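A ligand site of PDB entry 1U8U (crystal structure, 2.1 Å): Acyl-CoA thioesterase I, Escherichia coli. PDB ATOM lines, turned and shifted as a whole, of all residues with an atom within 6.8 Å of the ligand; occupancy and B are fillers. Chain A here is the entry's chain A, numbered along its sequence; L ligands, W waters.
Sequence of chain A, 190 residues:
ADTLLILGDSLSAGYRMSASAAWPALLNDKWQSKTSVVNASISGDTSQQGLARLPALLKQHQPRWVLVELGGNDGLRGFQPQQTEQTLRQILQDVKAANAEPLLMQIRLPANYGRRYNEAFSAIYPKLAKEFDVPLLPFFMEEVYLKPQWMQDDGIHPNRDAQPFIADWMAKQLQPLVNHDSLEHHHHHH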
ATOM      1  N   GLY A   8      24.045  22.003 -21.123  1.00  0.00           N
ATOM      2  CA  GLY A   8      22.932  21.342 -20.461  1.00  0.00           C
ATOM      3  C   GLY A   8      22.791  19.865 -20.753  1.00  0.00           C
ATOM      4  O   GLY A   8      23.669  19.237 -21.319  1.00  0.00           O
ATOM      5  N   ASP A   9      21.664  19.314 -20.339  1.00  0.00           N
ATOM      6  CA  ASP A   9      21.377  17.888 -20.510  1.00  0.00           C
ATOM      7  C   ASP A   9      20.246  17.626 -21.503  1.00  0.00           C
ATOM      8  O   ASP A   9      20.040  18.391 -22.450  1.00  0.00           O
ATOM      9  CB  ASP A   9      21.082  17.244 -19.131  1.00  0.00           C
ATOM     10  CG  ASP A   9      20.044  18.023 -18.309  1.00  0.00           C
ATOM     11  OD1 ASP A   9      19.072  18.541 -18.892  1.00  0.00           O
ATOM     12  OD2 ASP A   9      20.179  18.086 -17.056  1.00  0.00           O
ATOM     13  N   SER A  10      19.537  16.518 -21.319  1.00  0.00           N
ATOM     14  CA  SER A  10      18.490  16.209 -22.268  1.00  0.00           C
ATOM     15  C   SER A  10      17.454  17.319 -22.402  1.00  0.00           C
ATOM     16  O   SER A  10      16.884  17.516 -23.478  1.00  0.00           O
ATOM     17  CB  SER A  10      17.817  14.898 -21.884  1.00  0.00           C
ATOM     18  OG  SER A  10      16.878  14.520 -22.870  1.00  0.00           O
ATOM     19  N   LEU A  11      17.215  18.057 -21.327  1.00  0.00           N
ATOM     20  CA  LEU A  11      16.229  19.108 -21.452  1.00  0.00           C
ATOM     21  C   LEU A  11      16.599  20.078 -22.556  1.00  0.00           C
ATOM     22  O   LEU A  11      15.716  20.661 -23.182  1.00  0.00           O
ATOM     23  CB  LEU A  11      16.026  19.835 -20.117  1.00  0.00           C
ATOM     24  CG  LEU A  11      15.399  18.984 -18.987  1.00  0.00           C
ATOM     25  CD1 LEU A  11      15.141  19.898 -17.828  1.00  0.00           C
ATOM     26  CD2 LEU A  11      14.075  18.295 -19.419  1.00  0.00           C
ATOM     27  N   SER A  12      17.890  20.247 -22.815  1.00  0.00           N
ATOM     28  CA  SER A  12      18.355  21.131 -23.868  1.00  0.00           C
ATOM     29  C   SER A  12      18.792  20.391 -25.122  1.00  0.00           C
ATOM     30  O   SER A  12      18.642  20.895 -26.225  1.00  0.00           O
ATOM     31  CB  SER A  12      19.487  22.025 -23.372  1.00  0.00           C
ATOM     32  OG  SER A  12      18.986  22.913 -22.381  1.00  0.00           O
ATOM     33  N   TYR A  15      15.241  14.861 -25.850  1.00  0.00           N
ATOM     34  CA  TYR A  15      15.181  13.474 -25.425  1.00  0.00           C
ATOM     35  C   TYR A  15      14.423  12.635 -26.452  1.00  0.00           C
ATOM     36  O   TYR A  15      13.241  12.871 -26.710  1.00  0.00           O
ATOM     37  CB  TYR A  15      14.520  13.387 -24.055  1.00  0.00           C
ATOM     38  CG  TYR A  15      14.458  12.001 -23.486  1.00  0.00           C
ATOM     39  CD1 TYR A  15      13.288  11.249 -23.539  1.00  0.00           C
ATOM     40  CD2 TYR A  15      15.589  11.445 -22.859  1.00  0.00           C
ATOM     41  CE1 TYR A  15      13.228   9.977 -22.989  1.00  0.00           C
ATOM     42  CE2 TYR A  15      15.536  10.179 -22.299  1.00  0.00           C
ATOM     43  CZ  TYR A  15      14.364   9.442 -22.369  1.00  0.00           C
ATOM     44  OH  TYR A  15      14.312   8.188 -21.817  1.00  0.00           O
ATOM     45  N   ILE A  42      24.106  17.150 -23.602  1.00  0.00           N
ATOM     46  CA  ILE A  42      24.076  15.712 -23.843  1.00  0.00           C
ATOM     47  C   ILE A  42      23.074  15.066 -22.884  1.00  0.00           C
ATOM     48  O   ILE A  42      23.078  15.356 -21.680  1.00  0.00           O
ATOM     49  CB  ILE A  42      25.480  15.120 -23.630  1.00  0.00           C
ATOM     50  CG1 ILE A  42      26.501  15.856 -24.502  1.00  0.00           C
ATOM     51  CG2 ILE A  42      25.497  13.638 -23.957  1.00  0.00           C
ATOM     52  CD1 ILE A  42      27.935  15.433 -24.247  1.00  0.00           C
ATOM     53  N   SER A  43      22.232  14.181 -23.400  1.00  0.00           N
ATOM     54  CA  SER A  43      21.267  13.518 -22.524  1.00  0.00           C
ATOM     55  C   SER A  43      21.984  12.702 -21.449  1.00  0.00           C
ATOM     56  O   SER A  43      23.014  12.069 -21.716  1.00  0.00           O
ATOM     57  CB  SER A  43      20.365  12.593 -23.330  1.00  0.00           C
ATOM     58  OG  SER A  43      19.530  13.354 -24.183  1.00  0.00           O
ATOM     59  N   GLY A  44      21.443  12.736 -20.227  1.00  0.00           N
ATOM     60  CA  GLY A  44      22.003  12.000 -19.106  1.00  0.00           C
ATOM     61  C   GLY A  44      23.184  12.618 -18.415  1.00  0.00           C
ATOM     62  O   GLY A  44      23.661  12.086 -17.422  1.00  0.00           O
ATOM     63  N   ASP A  45      23.670  13.746 -18.913  1.00  0.00           N
ATOM     64  CA  ASP A  45      24.830  14.412 -18.332  1.00  0.00           C
ATOM     65  C   ASP A  45      24.557  14.952 -16.933  1.00  0.00           C
ATOM     66  O   ASP A  45      23.612  15.721 -16.730  1.00  0.00           O
ATOM     67  CB  ASP A  45      25.288  15.586 -19.204  1.00  0.00           C
ATOM     68  CG  ASP A  45      26.632  15.337 -19.911  1.00  0.00           C
ATOM     69  OD1 ASP A  45      27.416  16.296 -20.080  1.00  0.00           O
ATOM     70  OD2 ASP A  45      26.900  14.197 -20.327  1.00  0.00           O
ATOM     71  N   THR A  46      25.398  14.541 -15.972  1.00  0.00           N
ATOM     72  CA  THR A  46      25.307  15.042 -14.604  1.00  0.00           C
ATOM     73  C   THR A  46      26.039  16.382 -14.613  1.00  0.00           C
ATOM     74  O   THR A  46      26.632  16.764 -15.636  1.00  0.00           O
ATOM     75  CB  THR A  46      26.054  14.135 -13.612  1.00  0.00           C
ATOM     76  OG1 THR A  46      27.445  14.101 -13.959  1.00  0.00           O
ATOM     77  CG2 THR A  46      25.506  12.712 -13.637  1.00  0.00           C
ATOM     78  N   GLU A  69      22.391  24.712 -17.663  1.00  0.00           N
ATOM     79  CA  GLU A  69      21.178  23.940 -17.365  1.00  0.00           C
ATOM     80  C   GLU A  69      21.600  22.527 -16.971  1.00  0.00           C
ATOM     81  O   GLU A  69      21.536  21.604 -17.779  1.00  0.00           O
ATOM     82  CB  GLU A  69      20.272  23.931 -18.600  1.00  0.00           C
ATOM     83  CG  GLU A  69      18.937  23.223 -18.416  1.00  0.00           C
ATOM     84  CD  GLU A  69      18.981  21.755 -18.847  1.00  0.00           C
ATOM     85  OE1 GLU A  69      18.558  20.889 -18.046  1.00  0.00           O
ATOM     86  OE2 GLU A  69      19.430  21.472 -19.973  1.00  0.00           O
ATOM     87  N   GLY A  71      22.202  19.646 -13.282  1.00  0.00           N
ATOM     88  CA  GLY A  71      21.883  19.293 -11.904  1.00  0.00           C
ATOM     89  C   GLY A  71      20.701  18.347 -11.815  1.00  0.00           C
ATOM     90  O   GLY A  71      20.600  17.542 -10.884  1.00  0.00           O
ATOM     91  N   GLY A  72      19.789  18.446 -12.782  1.00  0.00           N
ATOM     92  CA  GLY A  72      18.607  17.603 -12.781  1.00  0.00           C
ATOM     93  C   GLY A  72      18.864  16.104 -12.711  1.00  0.00           C
ATOM     94  O   GLY A  72      18.123  15.378 -12.054  1.00  0.00           O
ATOM     95  N   ASN A  73      19.899  15.620 -13.396  1.00  0.00           N
ATOM     96  CA  ASN A  73      20.191  14.189 -13.360  1.00  0.00           C
ATOM     97  C   ASN A  73      20.766  13.799 -11.982  1.00  0.00           C
ATOM     98  O   ASN A  73      20.504  12.699 -11.485  1.00  0.00           O
ATOM     99  CB  ASN A  73      21.171  13.771 -14.469  1.00  0.00           C
ATOM    100  CG  ASN A  73      20.526  13.792 -15.850  1.00  0.00           C
ATOM    101  OD1 ASN A  73      19.460  13.185 -16.081  1.00  0.00           O
ATOM    102  ND2 ASN A  73      21.178  14.480 -16.787  1.00  0.00           N
ATOM    103  N   LEU A  76      17.942  13.693  -9.607  1.00  0.00           N
ATOM    104  CA  LEU A  76      17.108  12.578 -10.032  1.00  0.00           C
ATOM    105  C   LEU A  76      17.732  11.260  -9.568  1.00  0.00           C
ATOM    106  O   LEU A  76      17.019  10.297  -9.293  1.00  0.00           O
ATOM    107  CB  LEU A  76      16.985  12.594 -11.551  1.00  0.00           C
ATOM    108  CG  LEU A  76      15.626  12.284 -12.162  1.00  0.00           C
ATOM    109  CD1 LEU A  76      14.564  13.238 -11.618  1.00  0.00           C
ATOM    110  CD2 LEU A  76      15.733  12.402 -13.684  1.00  0.00           C
ATOM    111  N   ILE A 107      16.644  24.577 -11.443  1.00  0.00           N
ATOM    112  CA  ILE A 107      16.149  23.217 -11.687  1.00  0.00           C
ATOM    113  C   ILE A 107      15.346  22.719 -10.485  1.00  0.00           C
ATOM    114  O   ILE A 107      15.719  23.006  -9.321  1.00  0.00           O
ATOM    115  CB  ILE A 107      17.275  22.210 -11.927  1.00  0.00           C
ATOM    116  CG1 ILE A 107      18.218  22.691 -13.018  1.00  0.00           C
ATOM    117  CG2 ILE A 107      16.646  20.873 -12.350  1.00  0.00           C
ATOM    118  CD1 ILE A 107      17.508  22.908 -14.382  1.00  0.00           C
ATOM    119  N   ARG A 108      14.278  21.960 -10.740  1.00  0.00           N
ATOM    120  CA  ARG A 108      13.423  21.420  -9.688  1.00  0.00           C
ATOM    121  C   ARG A 108      13.100  19.954  -9.925  1.00  0.00           C
ATOM    122  O   ARG A 108      12.888  19.541 -11.062  1.00  0.00           O
ATOM    123  CB  ARG A 108      12.113  22.209  -9.573  1.00  0.00           C
ATOM    124  CG  ARG A 108      12.345  23.604  -9.018  1.00  0.00           C
ATOM    125  CD  ARG A 108      11.115  24.522  -9.045  1.00  0.00           C
ATOM    126  NE  ARG A 108      11.428  25.797  -8.390  1.00  0.00           N
ATOM    127  CZ  ARG A 108      11.687  25.905  -7.088  1.00  0.00           C
ATOM    128  NH1 ARG A 108      11.640  24.828  -6.306  1.00  0.00           N
ATOM    129  NH2 ARG A 108      12.017  27.079  -6.559  1.00  0.00           N
ATOM    130  N   LEU A 109      13.068  19.184  -8.853  1.00  0.00           N
ATOM    131  CA  LEU A 109      12.806  17.757  -8.945  1.00  0.00           C
ATOM    132  C   LEU A 109      11.336  17.434  -8.804  1.00  0.00           C
ATOM    133  O   LEU A 109      10.540  18.256  -8.382  1.00  0.00           O
ATOM    134  CB  LEU A 109      13.607  17.002  -7.869  1.00  0.00           C
ATOM    135  CG  LEU A 109      15.136  17.177  -7.956  1.00  0.00           C
ATOM    136  CD1 LEU A 109      15.793  16.342  -6.866  1.00  0.00           C
ATOM    137  CD2 LEU A 109      15.636  16.738  -9.336  1.00  0.00           C
ATOM    138  N   PRO A 110      10.967  16.198  -9.163  1.00  0.00           N
ATOM    139  CA  PRO A 110       9.568  15.768  -9.058  1.00  0.00           C
ATOM    140  C   PRO A 110       9.130  15.772  -7.593  1.00  0.00           C
ATOM    141  O   PRO A 110       9.937  15.499  -6.699  1.00  0.00           O
ATOM    142  CB  PRO A 110       9.587  14.383  -9.664  1.00  0.00           C
ATOM    143  CG  PRO A 110      10.690  14.474 -10.678  1.00  0.00           C
ATOM    144  CD  PRO A 110      11.751  15.220  -9.927  1.00  0.00           C
ATOM    145  N   PHE A 121      17.936  20.522  -2.810  1.00  0.00           N
ATOM    146  CA  PHE A 121      18.360  20.548  -4.206  1.00  0.00           C
ATOM    147  C   PHE A 121      18.042  21.929  -4.800  1.00  0.00           C
ATOM    148  O   PHE A 121      18.940  22.629  -5.255  1.00  0.00           O
ATOM    149  CB  PHE A 121      17.619  19.480  -5.024  1.00  0.00           C
ATOM    150  CG  PHE A 121      17.979  19.491  -6.491  1.00  0.00           C
ATOM    151  CD1 PHE A 121      19.198  18.993  -6.924  1.00  0.00           C
ATOM    152  CD2 PHE A 121      17.088  20.003  -7.446  1.00  0.00           C
ATOM    153  CE1 PHE A 121      19.547  19.014  -8.273  1.00  0.00           C
ATOM    154  CE2 PHE A 121      17.426  20.030  -8.801  1.00  0.00           C
ATOM    155  CZ  PHE A 121      18.664  19.532  -9.218  1.00  0.00           C
ATOM    156  N   PHE A 139      12.639  27.883 -14.167  1.00  0.00           N
ATOM    157  CA  PHE A 139      12.719  26.533 -14.750  1.00  0.00           C
ATOM    158  C   PHE A 139      11.662  26.404 -15.826  1.00  0.00           C
ATOM    159  O   PHE A 139      10.478  26.287 -15.510  1.00  0.00           O
ATOM    160  CB  PHE A 139      12.509  25.484 -13.638  1.00  0.00           C
ATOM    161  CG  PHE A 139      12.764  24.039 -14.068  1.00  0.00           C
ATOM    162  CD1 PHE A 139      13.702  23.724 -15.053  1.00  0.00           C
ATOM    163  CD2 PHE A 139      12.095  22.989 -13.427  1.00  0.00           C
ATOM    164  CE1 PHE A 139      13.984  22.395 -15.379  1.00  0.00           C
ATOM    165  CE2 PHE A 139      12.351  21.650 -13.747  1.00  0.00           C
ATOM    166  CZ  PHE A 139      13.301  21.350 -14.720  1.00  0.00           C
ATOM    167  N   MET A 141      10.567  24.026 -17.528  1.00  0.00           N
ATOM    168  CA  MET A 141       9.708  22.845 -17.425  1.00  0.00           C
ATOM    169  C   MET A 141       8.414  23.103 -16.644  1.00  0.00           C
ATOM    170  O   MET A 141       7.412  22.421 -16.876  1.00  0.00           O
ATOM    171  CB  MET A 141      10.455  21.654 -16.787  1.00  0.00           C
ATOM    172  CG  MET A 141      11.365  20.915 -17.763  1.00  0.00           C
ATOM    173  SD  MET A 141      10.536  20.667 -19.375  1.00  0.00           S
ATOM    174  CE  MET A 141       9.434  19.198 -19.113  1.00  0.00           C
ATOM    175  N   TYR A 145       4.861  21.318 -17.798  1.00  0.00           N
ATOM    176  CA  TYR A 145       4.107  20.381 -16.960  1.00  0.00           C
ATOM    177  C   TYR A 145       2.616  20.656 -17.011  1.00  0.00           C
ATOM    178  O   TYR A 145       1.803  19.775 -16.819  1.00  0.00           O
ATOM    179  CB  TYR A 145       4.553  20.521 -15.492  1.00  0.00           C
ATOM    180  CG  TYR A 145       5.929  20.044 -15.212  1.00  0.00           C
ATOM    181  CD1 TYR A 145       6.668  20.561 -14.147  1.00  0.00           C
ATOM    182  CD2 TYR A 145       6.528  19.071 -16.021  1.00  0.00           C
ATOM    183  CE1 TYR A 145       7.967  20.125 -13.892  1.00  0.00           C
ATOM    184  CE2 TYR A 145       7.826  18.635 -15.767  1.00  0.00           C
ATOM    185  CZ  TYR A 145       8.530  19.160 -14.709  1.00  0.00           C
ATOM    186  OH  TYR A 145       9.815  18.735 -14.491  1.00  0.00           O
ATOM    187  N   GLY A 155       6.848  11.433 -18.137  1.00  0.00           N
ATOM    188  CA  GLY A 155       6.429  12.499 -17.251  1.00  0.00           C
ATOM    189  C   GLY A 155       7.607  13.364 -16.857  1.00  0.00           C
ATOM    190  O   GLY A 155       7.514  14.191 -15.948  1.00  0.00           O
ATOM    191  N   ILE A 156       8.712  13.196 -17.567  1.00  0.00           N
ATOM    192  CA  ILE A 156       9.912  13.964 -17.265  1.00  0.00           C
ATOM    193  C   ILE A 156      10.371  14.844 -18.428  1.00  0.00           C
ATOM    194  O   ILE A 156      10.687  16.022 -18.256  1.00  0.00           O
ATOM    195  CB  ILE A 156      11.070  13.018 -16.891  1.00  0.00           C
ATOM    196  CG1 ILE A 156      10.718  12.258 -15.607  1.00  0.00           C
ATOM    197  CG2 ILE A 156      12.372  13.804 -16.741  1.00  0.00           C
ATOM    198  CD1 ILE A 156      11.706  11.164 -15.264  1.00  0.00           C
ATOM    199  N   HIS A 157      10.402  14.279 -19.619  1.00  0.00           N
ATOM    200  CA  HIS A 157      10.899  15.004 -20.766  1.00  0.00           C
ATOM    201  C   HIS A 157       9.854  15.615 -21.660  1.00  0.00           C
ATOM    202  O   HIS A 157       8.795  15.019 -21.911  1.00  0.00           O
ATOM    203  CB  HIS A 157      11.821  14.101 -21.577  1.00  0.00           C
ATOM    204  CG  HIS A 157      12.907  13.462 -20.773  1.00  0.00           C
ATOM    205  ND1 HIS A 157      12.824  12.177 -20.286  1.00  0.00           N
ATOM    206  CD2 HIS A 157      14.124  13.927 -20.374  1.00  0.00           C
ATOM    207  CE1 HIS A 157      13.937  11.872 -19.640  1.00  0.00           C
ATOM    208  NE2 HIS A 157      14.735  12.916 -19.677  1.00  0.00           N
HETATM  209  C1  LIG L   1      18.185  14.383 -18.840  1.00  0.00           C
HETATM  210  C2  LIG L   1      17.388  15.506 -18.181  1.00  0.00           C
HETATM  211  C3  LIG L   1      17.244  15.495 -16.656  1.00  0.00           C
HETATM  212  C4  LIG L   1      15.876  16.056 -16.318  1.00  0.00           C
HETATM  213  C5  LIG L   1      15.856  16.655 -14.932  1.00  0.00           C
HETATM  214  C6  LIG L   1      14.654  17.532 -14.617  1.00  0.00           C
HETATM  215  C7  LIG L   1      14.072  17.218 -13.257  1.00  0.00           C
HETATM  216  C8  LIG L   1      12.635  16.646 -13.206  1.00  0.00           C
HETATM  217  O1  LIG L   1      17.471  13.313 -19.051  1.00  0.00           O
HETATM  218  O2  LIG L   1      19.421  14.577 -19.162  1.00  0.00           O
HETATM  219  O   HOH W   1      11.010  17.059 -15.726  1.00  0.00           O
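A ring nitrogen (NE2) of His 157 sits at hydrogen-bond distance from an oxygen (O1) of the ligand, 2.8 Å away.
The backbone NH of Ser 10 is in hydrogen-bond range of an oxygen (O2) of the ligand (2.9 Å).
N of Gly 44 sits at hydrogen-bond distance from O2 of the ligand (2.9 Å).
The side-chain amide nitrogen of Asn 73 lies within hydrogen-bond range of an oxygen (O2) of the ligand, 3.0 Å away.
OG of Ser 43 sits at hydrogen-bond distance from OG of Ser 10 (3.2 Å).
The backbone NH (N) of Tyr 15 sits close to the side-chain hydroxyl (OG) of Ser 10 (3.4 Å).
The side-chain amide nitrogen (ND2) of Asn 73 lies within hydrogen-bond range of the backbone carbonyl oxygen (O) of Asp 45 (2.7 Å).
The side-chain carboxylate (OD1) of Asp 9 lies close to the backbone NH (N) of Leu 11, at 3.1 Å.
The backbone NH (N) of Asp 9 is in hydrogen-bond range of the side-chain carboxylate (OE2) of Glu 69 (3.1 Å).
Merely in contact with the ligand: Asp 9 (3.1 Å), Leu 11 (3.99 Å), Ser 43 (3.9 Å), Gly 72 (3.6 Å), Arg 108 (3.4 Å), Pro 110 (3.7 Å) and Tyr 145 (3.7 Å).
11 residues have an atom within 4 Å of the ligand: Asp 9, Ser 10, Leu 11, Ser 43, Gly 44, Gly 72, Asn 73, Arg 108, Pro 110, Tyr 145 and His 157.
Water W1 bridges the side-chain hydroxyl of Tyr 145 (2.4 Å) and the backbone carbonyl oxygen of Ile 156 (2.8 Å).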
